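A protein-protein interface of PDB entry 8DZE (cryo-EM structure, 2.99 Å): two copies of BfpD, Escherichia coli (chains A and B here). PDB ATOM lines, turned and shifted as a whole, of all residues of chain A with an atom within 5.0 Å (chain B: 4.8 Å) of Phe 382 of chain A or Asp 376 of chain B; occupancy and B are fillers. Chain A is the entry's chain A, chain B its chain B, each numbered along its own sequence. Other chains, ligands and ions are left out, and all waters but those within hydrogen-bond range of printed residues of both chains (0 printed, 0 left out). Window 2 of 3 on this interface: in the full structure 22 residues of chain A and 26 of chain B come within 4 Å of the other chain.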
ATOM      1  N   THR A 350     -19.521  -3.222  20.323  1.00  0.00           N
ATOM      2  CA  THR A 350     -19.318  -4.655  20.133  1.00  0.00           C
ATOM      3  C   THR A 350     -17.847  -5.031  20.247  1.00  0.00           C
ATOM      4  O   THR A 350     -17.522  -6.103  20.767  1.00  0.00           O
ATOM      5  CB  THR A 350     -19.872  -5.110  18.782  1.00  0.00           C
ATOM      6  OG1 THR A 350     -19.275  -4.339  17.731  1.00  0.00           O
ATOM      7  CG2 THR A 350     -21.385  -4.957  18.740  1.00  0.00           C
ATOM      8  N   ASP A 380     -28.864   0.846  23.526  1.00  0.00           N
ATOM      9  CA  ASP A 380     -29.749  -0.003  24.329  1.00  0.00           C
ATOM     10  C   ASP A 380     -29.308  -0.056  25.788  1.00  0.00           C
ATOM     11  O   ASP A 380     -28.131   0.142  26.104  1.00  0.00           O
ATOM     12  CB  ASP A 380     -29.870  -1.422  23.754  1.00  0.00           C
ATOM     13  CG  ASP A 380     -30.548  -1.447  22.400  1.00  0.00           C
ATOM     14  OD1 ASP A 380     -31.733  -1.060  22.319  1.00  0.00           O
ATOM     15  OD2 ASP A 380     -29.898  -1.856  21.416  1.00  0.00           O
ATOM     16  N   GLU A 381     -30.259  -0.325  26.686  1.00  0.00           N
ATOM     17  CA  GLU A 381     -30.021  -0.159  28.115  1.00  0.00           C
ATOM     18  C   GLU A 381     -29.138  -1.252  28.706  1.00  0.00           C
ATOM     19  O   GLU A 381     -28.423  -0.996  29.681  1.00  0.00           O
ATOM     20  CB  GLU A 381     -31.354  -0.113  28.865  1.00  0.00           C
ATOM     21  N   PHE A 382     -29.172  -2.466  28.152  1.00  0.00           N
ATOM     22  CA  PHE A 382     -28.418  -3.559  28.757  1.00  0.00           C
ATOM     23  C   PHE A 382     -26.915  -3.424  28.538  1.00  0.00           C
ATOM     24  O   PHE A 382     -26.138  -4.003  29.304  1.00  0.00           O
ATOM     25  CB  PHE A 382     -28.919  -4.911  28.232  1.00  0.00           C
ATOM     26  CG  PHE A 382     -28.636  -5.156  26.774  1.00  0.00           C
ATOM     27  CD1 PHE A 382     -29.512  -4.707  25.799  1.00  0.00           C
ATOM     28  CD2 PHE A 382     -27.514  -5.868  26.379  1.00  0.00           C
ATOM     29  CE1 PHE A 382     -29.262  -4.938  24.460  1.00  0.00           C
ATOM     30  CE2 PHE A 382     -27.258  -6.103  25.042  1.00  0.00           C
ATOM     31  CZ  PHE A 382     -28.133  -5.638  24.082  1.00  0.00           C
ATOM     32  N   LYS A 383     -26.489  -2.680  27.516  1.00  0.00           N
ATOM     33  CA  LYS A 383     -25.064  -2.457  27.310  1.00  0.00           C
ATOM     34  C   LYS A 383     -24.498  -1.420  28.273  1.00  0.00           C
ATOM     35  O   LYS A 383     -23.337  -1.532  28.682  1.00  0.00           O
ATOM     36  CB  LYS A 383     -24.798  -2.025  25.867  1.00  0.00           C
ATOM     37  CG  LYS A 383     -25.048  -3.112  24.836  1.00  0.00           C
ATOM     38  CD  LYS A 383     -24.605  -2.668  23.454  1.00  0.00           C
ATOM     39  CE  LYS A 383     -24.933  -3.717  22.405  1.00  0.00           C
ATOM     40  NZ  LYS A 383     -24.530  -3.278  21.041  1.00  0.00           N
ATOM     41  N   LEU A 384     -25.292  -0.415  28.642  1.00  0.00           N
ATOM     42  CA  LEU A 384     -24.816   0.666  29.494  1.00  0.00           C
ATOM     43  C   LEU A 384     -24.873   0.336  30.980  1.00  0.00           C
ATOM     44  O   LEU A 384     -24.327   1.098  31.785  1.00  0.00           O
ATOM     45  CB  LEU A 384     -25.627   1.936  29.226  1.00  0.00           C
ATOM     46  CG  LEU A 384     -25.668   2.418  27.776  1.00  0.00           C
ATOM     47  CD1 LEU A 384     -26.944   3.195  27.503  1.00  0.00           C
ATOM     48  CD2 LEU A 384     -24.445   3.262  27.458  1.00  0.00           C
ATOM     49  N   THR A 385     -25.518  -0.765  31.364  1.00  0.00           N
ATOM     50  CA  THR A 385     -25.655  -1.098  32.778  1.00  0.00           C
ATOM     51  C   THR A 385     -24.367  -1.672  33.362  1.00  0.00           C
ATOM     52  O   THR A 385     -24.079  -1.456  34.546  1.00  0.00           O
ATOM     53  CB  THR A 385     -26.813  -2.080  32.968  1.00  0.00           C
ATOM     54  OG1 THR A 385     -27.968  -1.593  32.275  1.00  0.00           O
ATOM     55  CG2 THR A 385     -27.165  -2.230  34.442  1.00  0.00           C
ATOM     56  N   ASP A 386     -23.581  -2.376  32.558  1.00  0.00           N
ATOM     57  CA  ASP A 386     -22.382  -3.053  33.048  1.00  0.00           C
ATOM     58  C   ASP A 386     -21.306  -2.044  33.433  1.00  0.00           C
ATOM     59  O   ASP A 386     -20.883  -1.251  32.583  1.00  0.00           O
ATOM     60  CB  ASP A 386     -21.850  -4.003  31.977  1.00  0.00           C
ATOM     61  CG  ASP A 386     -21.145  -5.212  32.563  1.00  0.00           C
ATOM     62  OD1 ASP A 386     -20.820  -5.194  33.767  1.00  0.00           O
ATOM     63  OD2 ASP A 386     -20.913  -6.185  31.813  1.00  0.00           O
ATOM     64  N   ASP B 372     -25.113 -10.874  27.910  1.00  0.00           N
ATOM     65  CA  ASP B 372     -25.166  -9.597  27.204  1.00  0.00           C
ATOM     66  C   ASP B 372     -24.818  -9.754  25.729  1.00  0.00           C
ATOM     67  O   ASP B 372     -25.406  -9.073  24.880  1.00  0.00           O
ATOM     68  CB  ASP B 372     -24.229  -8.589  27.867  1.00  0.00           C
ATOM     69  CG  ASP B 372     -24.507  -8.423  29.347  1.00  0.00           C
ATOM     70  OD1 ASP B 372     -25.576  -8.876  29.807  1.00  0.00           O
ATOM     71  OD2 ASP B 372     -23.658  -7.835  30.051  1.00  0.00           O
ATOM     72  N   ARG B 373     -23.872 -10.635  25.405  1.00  0.00           N
ATOM     73  CA  ARG B 373     -23.525 -10.898  24.014  1.00  0.00           C
ATOM     74  C   ARG B 373     -24.588 -11.714  23.293  1.00  0.00           C
ATOM     75  O   ARG B 373     -24.658 -11.667  22.060  1.00  0.00           O
ATOM     76  CB  ARG B 373     -22.182 -11.627  23.934  1.00  0.00           C
ATOM     77  CG  ARG B 373     -20.988 -10.785  24.349  1.00  0.00           C
ATOM     78  CD  ARG B 373     -20.474  -9.949  23.191  1.00  0.00           C
ATOM     79  NE  ARG B 373     -20.072 -10.775  22.058  1.00  0.00           N
ATOM     80  CZ  ARG B 373     -20.226 -10.429  20.789  1.00  0.00           C
ATOM     81  NH1 ARG B 373     -20.775  -9.273  20.448  1.00  0.00           N
ATOM     82  NH2 ARG B 373     -19.821 -11.262  19.835  1.00  0.00           N
ATOM     83  N   LEU B 374     -25.409 -12.460  24.032  1.00  0.00           N
ATOM     84  CA  LEU B 374     -26.480 -13.243  23.428  1.00  0.00           C
ATOM     85  C   LEU B 374     -27.759 -12.433  23.244  1.00  0.00           C
ATOM     86  O   LEU B 374     -28.419 -12.552  22.207  1.00  0.00           O
ATOM     87  CB  LEU B 374     -26.766 -14.485  24.275  1.00  0.00           C
ATOM     88  CG  LEU B 374     -25.728 -15.608  24.209  1.00  0.00           C
ATOM     89  CD1 LEU B 374     -26.114 -16.753  25.130  1.00  0.00           C
ATOM     90  CD2 LEU B 374     -25.561 -16.099  22.783  1.00  0.00           C
ATOM     91  N   LYS B 375     -28.119 -11.603  24.226  1.00  0.00           N
ATOM     92  CA  LYS B 375     -29.306 -10.763  24.105  1.00  0.00           C
ATOM     93  C   LYS B 375     -29.158  -9.702  23.023  1.00  0.00           C
ATOM     94  O   LYS B 375     -30.170  -9.195  22.528  1.00  0.00           O
ATOM     95  CB  LYS B 375     -29.619 -10.090  25.442  1.00  0.00           C
ATOM     96  CG  LYS B 375     -30.142 -11.032  26.510  1.00  0.00           C
ATOM     97  CD  LYS B 375     -30.635 -10.263  27.723  1.00  0.00           C
ATOM     98  CE  LYS B 375     -29.475  -9.714  28.535  1.00  0.00           C
ATOM     99  NZ  LYS B 375     -29.935  -9.073  29.798  1.00  0.00           N
ATOM    100  N   ASP B 376     -27.925  -9.353  22.653  1.00  0.00           N
ATOM    101  CA  ASP B 376     -27.712  -8.379  21.589  1.00  0.00           C
ATOM    102  C   ASP B 376     -28.124  -8.931  20.230  1.00  0.00           C
ATOM    103  O   ASP B 376     -28.482  -8.160  19.332  1.00  0.00           O
ATOM    104  CB  ASP B 376     -26.244  -7.948  21.570  1.00  0.00           C
ATOM    105  CG  ASP B 376     -25.956  -6.888  20.526  1.00  0.00           C
ATOM    106  OD1 ASP B 376     -26.807  -5.994  20.332  1.00  0.00           O
ATOM    107  OD2 ASP B 376     -24.879  -6.950  19.897  1.00  0.00           O
ATOM    108  N   GLN B 377     -28.093 -10.253  20.061  1.00  0.00           N
ATOM    109  CA  GLN B 377     -28.329 -10.871  18.766  1.00  0.00           C
ATOM    110  C   GLN B 377     -29.689 -11.545  18.632  1.00  0.00           C
ATOM    111  O   GLN B 377     -30.028 -11.993  17.531  1.00  0.00           O
ATOM    112  CB  GLN B 377     -27.216 -11.886  18.464  1.00  0.00           C
ATOM    113  CG  GLN B 377     -25.843 -11.238  18.366  1.00  0.00           C
ATOM    114  CD  GLN B 377     -24.744 -12.229  18.052  1.00  0.00           C
ATOM    115  OE1 GLN B 377     -24.854 -13.410  18.364  1.00  0.00           O
ATOM    116  NE2 GLN B 377     -23.672 -11.748  17.432  1.00  0.00           N
ATOM    117  N   GLY B 378     -30.473 -11.633  19.705  1.00  0.00           N
ATOM    118  CA  GLY B 378     -31.842 -12.099  19.582  1.00  0.00           C
ATOM    119  C   GLY B 378     -32.130 -13.472  20.156  1.00  0.00           C
ATOM    120  O   GLY B 378     -32.950 -14.215  19.609  1.00  0.00           O
ATOM    121  N   ARG B 475     -27.394  -7.238  38.104  1.00  0.00           N
ATOM    122  CA  ARG B 475     -25.931  -7.170  38.110  1.00  0.00           C
ATOM    123  C   ARG B 475     -25.361  -6.999  39.517  1.00  0.00           C
ATOM    124  O   ARG B 475     -24.144  -6.883  39.690  1.00  0.00           O
ATOM    125  CB  ARG B 475     -25.416  -6.055  37.191  1.00  0.00           C
ATOM    126  CG  ARG B 475     -25.717  -6.274  35.719  1.00  0.00           C
ATOM    127  CD  ARG B 475     -25.013  -5.239  34.859  1.00  0.00           C
ATOM    128  NE  ARG B 475     -25.478  -5.265  33.479  1.00  0.00           N
ATOM    129  CZ  ARG B 475     -25.004  -6.076  32.543  1.00  0.00           C
ATOM    130  NH1 ARG B 475     -24.045  -6.948  32.807  1.00  0.00           N
ATOM    131  NH2 ARG B 475     -25.503  -6.009  31.312  1.00  0.00           N
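No position is printed for both chains.
Of the 7 pairs that touch across the chains among the printed residues, none has its exchanged pair printed and touching as well.
NH2 of Arg 475 of chain B is in salt-bridge range of OD2 of Asp 372 of chain B (2.9 Å).
OG1 of Thr 385 of chain A lies within hydrogen-bond range of O of Glu 381 of chain A, at 2.7 Å.
Among the printed residues, pairs that only touch across the chains: Phe 382 of chain A with Asp 372 of chain B, Phe 382 of chain A with Asp 376 of chain B, Thr 385 of chain A with Arg 475 of chain B and Asp 386 of chain A with Asp 372 of chain B.
The side-chain carboxylate of Asp 386 of chain A is in salt-bridge range of the guanidinium group of Arg 475 of chain B, 3.4 Å away.
The side-chain amino group (NZ) of Lys 383 of chain A is in salt-bridge range of the side-chain carboxylate (OD1) of Asp 376 of chain B (3.6 Å).
The backbone carbonyl oxygen of Phe 382 of chain A lies within hydrogen-bond range of the guanidinium group of Arg 475 of chain B (2.9 Å).
Of the 8 printed residues of chain A, 4 touch a printed residue of chain B.
Hydrophobic or aromatic side chains of chain A that line the printed part of chain B: Phe 382.
Among the printed residues, 7 pairs touch across the chains.
Of chain B, only Asp 372, Asp 376 and Arg 475 come within 4 Å of Phe 382 of chain A.
Printed residues of chain B within 4 Å of Lys 383 of chain A: Asp 376 (3.6 Å).
Printed residues of chain B within 4 Å of Asp 386 of chain A: Asp 372 and Arg 475.
Of the printed residues of chain A, Asp 372 of chain B touches Phe 382 (3.5 Å) and Asp 386 (3.7 Å).
Asp 376 of chain B touches just these residues of chain A: Phe 382 and Lys 383.
Of the printed residues of chain A, Arg 475 of chain B touches Phe 382, Thr 385 and Asp 386.
The nearest residue of chain B that does not touch Phe 382 of chain A is Lys 375 of chain B (4.3 Å).
The nearest printed residue of chain B that does not touch Thr 385 of chain A is Asp 372 of chain B (7.0 Å).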
